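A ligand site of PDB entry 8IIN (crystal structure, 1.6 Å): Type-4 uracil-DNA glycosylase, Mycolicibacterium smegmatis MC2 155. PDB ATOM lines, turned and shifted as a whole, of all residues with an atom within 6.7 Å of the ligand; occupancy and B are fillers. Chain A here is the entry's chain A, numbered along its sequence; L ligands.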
ATOM      1  N   GLY A   2       3.994 -20.957   8.661  1.00  0.00           N
ATOM      2  CA  GLY A   2       4.973 -20.546   7.659  1.00  0.00           C
ATOM      3  C   GLY A   2       4.384 -19.611   6.622  1.00  0.00           C
ATOM      4  O   GLY A   2       3.613 -18.689   6.929  1.00  0.00           O
ATOM      5  N   ALA A   3       4.729 -19.859   5.353  1.00  0.00           N
ATOM      6  CA  ALA A   3       4.287 -19.001   4.227  1.00  0.00           C
ATOM      7  C   ALA A   3       2.922 -19.366   3.690  1.00  0.00           C
ATOM      8  O   ALA A   3       2.483 -18.724   2.783  1.00  0.00           O
ATOM      9  CB  ALA A   3       5.257 -19.238   3.096  1.00  0.00           C
ATOM     10  N   PHE A   6       0.336 -16.791   2.741  1.00  0.00           N
ATOM     11  CA  PHE A   6       0.783 -15.798   1.773  1.00  0.00           C
ATOM     12  C   PHE A   6       0.732 -16.322   0.338  1.00  0.00           C
ATOM     13  O   PHE A   6       0.905 -15.526  -0.590  1.00  0.00           O
ATOM     14  CB  PHE A   6       2.205 -15.357   2.116  1.00  0.00           C
ATOM     15  CG  PHE A   6       2.311 -14.660   3.456  1.00  0.00           C
ATOM     16  CD1 PHE A   6       1.988 -13.323   3.595  1.00  0.00           C
ATOM     17  CD2 PHE A   6       2.716 -15.370   4.575  1.00  0.00           C
ATOM     18  CE1 PHE A   6       2.093 -12.680   4.840  1.00  0.00           C
ATOM     19  CE2 PHE A   6       2.818 -14.747   5.822  1.00  0.00           C
ATOM     20  CZ  PHE A   6       2.506 -13.403   5.950  1.00  0.00           C
ATOM     21  N   ALA A  20       5.010 -13.625  -3.491  1.00  0.00           N
ATOM     22  CA  ALA A  20       6.172 -13.933  -2.654  1.00  0.00           C
ATOM     23  C   ALA A  20       6.902 -12.664  -2.229  1.00  0.00           C
ATOM     24  O   ALA A  20       7.518 -12.637  -1.154  1.00  0.00           O
ATOM     25  CB  ALA A  20       7.116 -14.898  -3.379  1.00  0.00           C
ATOM     26  N   GLY A  21       6.839 -11.597  -3.027  1.00  0.00           N
ATOM     27  CA  GLY A  21       7.397 -10.321  -2.603  1.00  0.00           C
ATOM     28  C   GLY A  21       6.773  -9.802  -1.324  1.00  0.00           C
ATOM     29  O   GLY A  21       7.420  -9.030  -0.589  1.00  0.00           O
ATOM     30  N   GLU A  22       5.563 -10.250  -1.012  1.00  0.00           N
ATOM     31  CA  GLU A  22       4.859  -9.776   0.216  1.00  0.00           C
ATOM     32  C   GLU A  22       4.916 -10.818   1.345  1.00  0.00           C
ATOM     33  O   GLU A  22       4.296 -10.589   2.368  1.00  0.00           O
ATOM     34  CB  GLU A  22       3.399  -9.465  -0.120  1.00  0.00           C
ATOM     35  CG  GLU A  22       3.225  -8.616  -1.370  1.00  0.00           C
ATOM     36  CD  GLU A  22       3.803  -7.227  -1.224  1.00  0.00           C
ATOM     37  OE1 GLU A  22       3.727  -6.676  -0.109  1.00  0.00           O
ATOM     38  N   CYS A  23       5.650 -11.923   1.145  1.00  0.00           N
ATOM     39  CA  CYS A  23       5.671 -12.975   2.156  1.00  0.00           C
ATOM     40  C   CYS A  23       6.385 -12.510   3.412  1.00  0.00           C
ATOM     41  O   CYS A  23       7.426 -11.847   3.353  1.00  0.00           O
ATOM     42  CB  CYS A  23       6.360 -14.224   1.592  1.00  0.00           C
ATOM     43  SG  CYS A  23       6.262 -15.643   2.697  1.00  0.00           S
ATOM     44  N   ARG A  24       5.814 -12.874   4.568  1.00  0.00           N
ATOM     45  CA  ARG A  24       6.432 -12.702   5.887  1.00  0.00           C
ATOM     46  C   ARG A  24       6.459 -14.036   6.631  1.00  0.00           C
ATOM     47  O   ARG A  24       6.451 -14.073   7.857  1.00  0.00           O
ATOM     48  CB  ARG A  24       5.702 -11.627   6.697  1.00  0.00           C
ATOM     49  CG  ARG A  24       5.632 -10.258   6.011  1.00  0.00           C
ATOM     50  CD  ARG A  24       5.094  -9.145   6.948  1.00  0.00           C
ATOM     51  NE  ARG A  24       3.881  -9.570   7.651  1.00  0.00           N
ATOM     52  CZ  ARG A  24       2.675  -9.583   7.110  1.00  0.00           C
ATOM     53  NH1 ARG A  24       2.464  -9.209   5.852  1.00  0.00           N
ATOM     54  NH2 ARG A  24       1.637  -9.992   7.843  1.00  0.00           N
ATOM     55  N   GLY A  25       6.495 -15.147   5.872  1.00  0.00           N
ATOM     56  CA  GLY A  25       6.342 -16.489   6.414  1.00  0.00           C
ATOM     57  C   GLY A  25       7.442 -16.891   7.387  1.00  0.00           C
ATOM     58  O   GLY A  25       7.252 -17.827   8.172  1.00  0.00           O
ATOM     59  N   CYS A  26       8.575 -16.222   7.333  1.00  0.00           N
ATOM     60  CA  CYS A  26       9.638 -16.359   8.334  1.00  0.00           C
ATOM     61  C   CYS A  26      10.312 -15.006   8.479  1.00  0.00           C
ATOM     62  O   CYS A  26       9.852 -14.004   7.942  1.00  0.00           O
ATOM     63  CB  CYS A  26      10.582 -17.513   7.947  1.00  0.00           C
ATOM     64  SG  CYS A  26      11.788 -17.140   6.624  1.00  0.00           S
ATOM     65  N   GLY A  27      11.416 -14.970   9.224  1.00  0.00           N
ATOM     66  CA  GLY A  27      12.062 -13.682   9.460  1.00  0.00           C
ATOM     67  C   GLY A  27      12.932 -13.168   8.330  1.00  0.00           C
ATOM     68  O   GLY A  27      13.356 -12.015   8.372  1.00  0.00           O
ATOM     69  N   LEU A  28      13.200 -13.993   7.310  1.00  0.00           N
ATOM     70  CA  LEU A  28      14.259 -13.660   6.354  1.00  0.00           C
ATOM     71  C   LEU A  28      13.893 -12.500   5.428  1.00  0.00           C
ATOM     72  O   LEU A  28      14.795 -11.897   4.840  1.00  0.00           O
ATOM     73  CB  LEU A  28      14.615 -14.904   5.515  1.00  0.00           C
ATOM     74  CG  LEU A  28      15.239 -16.023   6.361  1.00  0.00           C
ATOM     75  CD1 LEU A  28      15.545 -17.256   5.472  1.00  0.00           C
ATOM     76  CD2 LEU A  28      16.509 -15.528   7.069  1.00  0.00           C
ATOM     77  N   TYR A  29      12.597 -12.158   5.291  1.00  0.00           N
ATOM     78  CA  TYR A  29      12.243 -11.057   4.402  1.00  0.00           C
ATOM     79  C   TYR A  29      12.763  -9.722   4.912  1.00  0.00           C
ATOM     80  O   TYR A  29      12.894  -8.777   4.128  1.00  0.00           O
ATOM     81  CB  TYR A  29      10.714 -10.955   4.248  1.00  0.00           C
ATOM     82  CG  TYR A  29      10.034 -10.392   5.484  1.00  0.00           C
ATOM     83  CD1 TYR A  29       9.719 -11.218   6.554  1.00  0.00           C
ATOM     84  CD2 TYR A  29       9.734  -9.033   5.579  1.00  0.00           C
ATOM     85  CE1 TYR A  29       9.100 -10.700   7.682  1.00  0.00           C
ATOM     86  CE2 TYR A  29       9.124  -8.518   6.696  1.00  0.00           C
ATOM     87  CZ  TYR A  29       8.806  -9.356   7.748  1.00  0.00           C
ATOM     88  OH  TYR A  29       8.205  -8.851   8.876  1.00  0.00           O
ATOM     89  N   ARG A  30      13.032  -9.630   6.208  1.00  0.00           N
ATOM     90  CA  ARG A  30      13.360  -8.306   6.790  1.00  0.00           C
ATOM     91  C   ARG A  30      14.676  -7.720   6.262  1.00  0.00           C
ATOM     92  O   ARG A  30      14.682  -6.561   5.852  1.00  0.00           O
ATOM     93  CB  ARG A  30      13.382  -8.399   8.314  1.00  0.00           C
ATOM     94  CG  ARG A  30      12.014  -8.637   8.932  1.00  0.00           C
ATOM     95  CD  ARG A  30      12.037  -9.197  10.334  1.00  0.00           C
ATOM     96  NE  ARG A  30      13.101 -10.159  10.522  1.00  0.00           N
ATOM     97  CZ  ARG A  30      13.309 -10.838  11.637  1.00  0.00           C
ATOM     98  NH2 ARG A  30      14.307 -11.692  11.724  1.00  0.00           N
ATOM     99  N   ALA A  35      12.338 -10.771  -2.412  1.00  0.00           N
ATOM    100  CA  ALA A  35      12.205 -12.218  -2.615  1.00  0.00           C
ATOM    101  C   ALA A  35      12.760 -12.526  -3.998  1.00  0.00           C
ATOM    102  O   ALA A  35      12.676 -11.694  -4.897  1.00  0.00           O
ATOM    103  CB  ALA A  35      10.768 -12.642  -2.546  1.00  0.00           C
ATOM    104  N   ALA A  91      15.089 -23.390  -2.313  1.00  0.00           N
ATOM    105  CA  ALA A  91      14.243 -23.879  -1.197  1.00  0.00           C
ATOM    106  C   ALA A  91      13.756 -22.686  -0.364  1.00  0.00           C
ATOM    107  O   ALA A  91      12.629 -22.725   0.124  1.00  0.00           O
ATOM    108  CB  ALA A  91      15.033 -24.844  -0.368  1.00  0.00           C
ATOM    109  N   VAL A  92      14.643 -21.709  -0.172  1.00  0.00           N
ATOM    110  CA  VAL A  92      14.332 -20.482   0.597  1.00  0.00           C
ATOM    111  C   VAL A  92      14.424 -19.303  -0.396  1.00  0.00           C
ATOM    112  O   VAL A  92      15.323 -19.345  -1.225  1.00  0.00           O
ATOM    113  CB  VAL A  92      15.257 -20.393   1.819  1.00  0.00           C
ATOM    114  CG1 VAL A  92      15.301 -19.017   2.449  1.00  0.00           C
ATOM    115  CG2 VAL A  92      14.845 -21.433   2.851  1.00  0.00           C
ATOM    116  N   LYS A  93      13.490 -18.337  -0.328  1.00  0.00           N
ATOM    117  CA  LYS A  93      13.395 -17.243  -1.341  1.00  0.00           C
ATOM    118  C   LYS A  93      13.938 -15.879  -0.887  1.00  0.00           C
ATOM    119  O   LYS A  93      13.961 -14.970  -1.690  1.00  0.00           O
ATOM    120  CB  LYS A  93      11.957 -17.256  -1.859  1.00  0.00           C
ATOM    121  CG  LYS A  93      11.697 -18.570  -2.587  1.00  0.00           C
ATOM    122  CD  LYS A  93      10.379 -18.747  -3.262  1.00  0.00           C
ATOM    123  CE  LYS A  93      10.481 -19.763  -4.380  1.00  0.00           C
ATOM    124  NZ  LYS A  93      10.809 -21.128  -3.880  1.00  0.00           N
ATOM    125  N   HIS A  94      14.422 -15.822   0.332  1.00  0.00           N
ATOM    126  CA  HIS A  94      15.076 -14.592   0.827  1.00  0.00           C
ATOM    127  C   HIS A  94      16.496 -14.930   1.300  1.00  0.00           C
ATOM    128  O   HIS A  94      16.669 -15.917   1.982  1.00  0.00           O
ATOM    129  CB  HIS A  94      14.302 -13.899   1.931  1.00  0.00           C
ATOM    130  CG  HIS A  94      13.231 -12.986   1.447  1.00  0.00           C
ATOM    131  ND1 HIS A  94      11.926 -13.301   1.576  1.00  0.00           N
ATOM    132  CD2 HIS A  94      13.260 -11.779   0.888  1.00  0.00           C
ATOM    133  CE1 HIS A  94      11.173 -12.358   1.081  1.00  0.00           C
ATOM    134  NE2 HIS A  94      11.967 -11.405   0.686  1.00  0.00           N
ATOM    135  N   PHE A  95      17.449 -14.114   0.904  1.00  0.00           N
ATOM    136  CA  PHE A  95      18.857 -14.320   1.280  1.00  0.00           C
ATOM    137  C   PHE A  95      19.056 -14.138   2.781  1.00  0.00           C
ATOM    138  O   PHE A  95      18.675 -13.105   3.316  1.00  0.00           O
ATOM    139  CB  PHE A  95      19.657 -13.304   0.453  1.00  0.00           C
ATOM    140  CG  PHE A  95      21.152 -13.246   0.609  1.00  0.00           C
ATOM    141  CD1 PHE A  95      21.903 -14.384   0.795  1.00  0.00           C
ATOM    142  CD2 PHE A  95      21.805 -12.035   0.521  1.00  0.00           C
ATOM    143  CE1 PHE A  95      23.277 -14.313   0.906  1.00  0.00           C
ATOM    144  CE2 PHE A  95      23.179 -11.963   0.642  1.00  0.00           C
ATOM    145  CZ  PHE A  95      23.919 -13.109   0.830  1.00  0.00           C
ATOM    146  N   GLU A 115      13.094 -22.492   8.792  1.00  0.00           N
ATOM    147  CA  GLU A 115      12.917 -21.557   7.642  1.00  0.00           C
ATOM    148  C   GLU A 115      12.587 -22.332   6.355  1.00  0.00           C
ATOM    149  O   GLU A 115      11.754 -21.892   5.606  1.00  0.00           O
ATOM    150  CB  GLU A 115      14.171 -20.686   7.486  1.00  0.00           C
ATOM    151  CG  GLU A 115      14.259 -19.623   8.567  1.00  0.00           C
ATOM    152  CD  GLU A 115      15.653 -19.093   8.850  1.00  0.00           C
ATOM    153  OE1 GLU A 115      16.610 -19.730   8.447  1.00  0.00           O
ATOM    154  OE2 GLU A 115      15.755 -18.043   9.478  1.00  0.00           O
ATOM    155  N   ALA A 118       9.071 -23.398   6.545  1.00  0.00           N
ATOM    156  CA  ALA A 118       8.177 -22.219   6.421  1.00  0.00           C
ATOM    157  C   ALA A 118       8.042 -21.834   4.956  1.00  0.00           C
ATOM    158  O   ALA A 118       6.972 -21.419   4.566  1.00  0.00           O
ATOM    159  CB  ALA A 118       8.778 -21.056   7.191  1.00  0.00           C
ATOM    160  N   CYS A 119       9.133 -21.959   4.198  1.00  0.00           N
ATOM    161  CA  CYS A 119       9.135 -21.487   2.785  1.00  0.00           C
ATOM    162  C   CYS A 119       8.624 -22.559   1.808  1.00  0.00           C
ATOM    163  O   CYS A 119       8.260 -22.213   0.693  1.00  0.00           O
ATOM    164  CB  CYS A 119      10.556 -21.046   2.442  1.00  0.00           C
ATOM    165  SG  CYS A 119      10.603 -19.826   1.093  1.00  0.00           S
ATOM    166  N   ARG A 120       8.627 -23.796   2.258  1.00  0.00           N
ATOM    167  CA  ARG A 120       8.250 -24.929   1.372  1.00  0.00           C
ATOM    168  C   ARG A 120       6.924 -24.713   0.647  1.00  0.00           C
ATOM    169  O   ARG A 120       6.821 -25.186  -0.478  1.00  0.00           O
ATOM    170  CB  ARG A 120       8.329 -26.259   2.133  1.00  0.00           C
ATOM    171  CG  ARG A 120       8.392 -27.486   1.226  1.00  0.00           C
ATOM    172  CD  ARG A 120       8.795 -28.699   2.025  1.00  0.00           C
ATOM    173  NE  ARG A 120       7.943 -28.863   3.192  1.00  0.00           N
ATOM    174  CZ  ARG A 120       8.217 -29.670   4.198  1.00  0.00           C
ATOM    175  NH1 ARG A 120       9.326 -30.382   4.180  1.00  0.00           N
ATOM    176  NH2 ARG A 120       7.392 -29.766   5.223  1.00  0.00           N
ATOM    177  N   PRO A 121       5.878 -24.097   1.239  1.00  0.00           N
ATOM    178  CA  PRO A 121       4.655 -23.808   0.490  1.00  0.00           C
ATOM    179  C   PRO A 121       4.908 -23.177  -0.886  1.00  0.00           C
ATOM    180  O   PRO A 121       4.173 -23.467  -1.779  1.00  0.00           O
ATOM    181  CB  PRO A 121       3.865 -22.870   1.421  1.00  0.00           C
ATOM    182  CG  PRO A 121       4.196 -23.404   2.774  1.00  0.00           C
ATOM    183  CD  PRO A 121       5.653 -23.765   2.663  1.00  0.00           C
ATOM    184  N   TRP A 122       5.928 -22.321  -0.978  1.00  0.00           N
ATOM    185  CA  TRP A 122       6.248 -21.725  -2.302  1.00  0.00           C
ATOM    186  C   TRP A 122       6.738 -22.813  -3.269  1.00  0.00           C
ATOM    187  O   TRP A 122       6.310 -22.796  -4.400  1.00  0.00           O
ATOM    188  CB  TRP A 122       7.245 -20.560  -2.180  1.00  0.00           C
ATOM    189  CG  TRP A 122       6.704 -19.365  -1.466  1.00  0.00           C
ATOM    190  CD1 TRP A 122       7.119 -18.860  -0.270  1.00  0.00           C
ATOM    191  CD2 TRP A 122       5.643 -18.519  -1.911  1.00  0.00           C
ATOM    192  NE1 TRP A 122       6.377 -17.766   0.064  1.00  0.00           N
ATOM    193  CE2 TRP A 122       5.460 -17.539  -0.926  1.00  0.00           C
ATOM    194  CE3 TRP A 122       4.818 -18.509  -3.040  1.00  0.00           C
ATOM    195  CZ2 TRP A 122       4.484 -16.549  -1.041  1.00  0.00           C
ATOM    196  CZ3 TRP A 122       3.861 -17.525  -3.166  1.00  0.00           C
ATOM    197  CH2 TRP A 122       3.695 -16.566  -2.169  1.00  0.00           C
HETATM  198 FE1  LIG L   1      10.338 -17.832   2.226  1.00  0.00          FE
HETATM  199 FE2  LIG L   1      10.598 -16.723   4.676  1.00  0.00          FE
HETATM  200 FE3  LIG L   1       8.505 -16.067   3.047  1.00  0.00          FE
HETATM  201 FE4  LIG L   1      11.006 -15.245   2.497  1.00  0.00          FE
HETATM  202  S1  LIG L   1       9.755 -14.641   4.344  1.00  0.00           S
HETATM  203  S2  LIG L   1       9.505 -16.128   0.993  1.00  0.00           S
HETATM  204  S3  LIG L   1      12.274 -17.021   3.111  1.00  0.00           S
HETATM  205  S4  LIG L   1       8.910 -18.105   4.022  1.00  0.00           S
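Residues that only touch the ligand: Ala 3 (3.9 Å), Leu 28 (3.97 Å), Tyr 29 (3.8 Å), Val 92 (3.7 Å), Lys 93 (3.9 Å) and Ala 118 (3.9 Å).
Hydrophobic or aromatic side chains within 4 Å of the ligand: Ala 3, Leu 28, Tyr 29, Val 92, His 94 and Trp 122.
Within 4 Å of the ligand: Ala 3, Cys 23, Gly 25, Cys 26, Leu 28, Tyr 29, Val 92, Lys 93, His 94, Ala 118, Cys 119 and Trp 122.
The side-chain sulfur (SG) of Cys 119 sits close to the backbone NH (N) of Lys 93, 3.5 Å away.
The backbone carbonyl oxygen of Ala 91 lies close to the side-chain sulfur of Cys 119, at 3.7 Å.
The side-chain sulfur (SG) of Cys 23 lies close to the backbone NH (N) of Gly 25 (3.2 Å).
The side-chain sulfur (SG) of Cys 23 lies close to the indole nitrogen (NE1) of Trp 122.
SG of Cys 26 sits close to N of Leu 28.
NE2 of His 94 sits at hydrogen-bond distance from N of Ala 35.
The backbone NH (N) of Ala 3 sits at hydrogen-bond distance from the backbone carbonyl oxygen (O) of Ala 118 (2.8 Å).
The side-chain sulfur (SG) of Cys 119 binds an iron atom (FE1) of the ligand (2.3 Å).
The side-chain sulfur (SG) of Cys 23 binds an iron atom (FE3) of the ligand, 2.3 Å away.
A sulfur (S1) of the ligand lies close to the backbone NH (N) of Cys 26.
An iron atom (FE2) of the ligand is bound by the side-chain sulfur of Cys 26 (2.3 Å).
The backbone NH of His 94 lies close to a sulfur (S3) of the ligand (3.7 Å).
An iron atom (FE4) of the ligand is bound by a ring nitrogen (ND1) of His 94, at 2.3 Å.
N of Gly 25 sits close to S1 of the ligand (3.6 Å).
The indole nitrogen of Trp 122 sits close to a sulfur (S2) of the ligand (3.7 Å).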
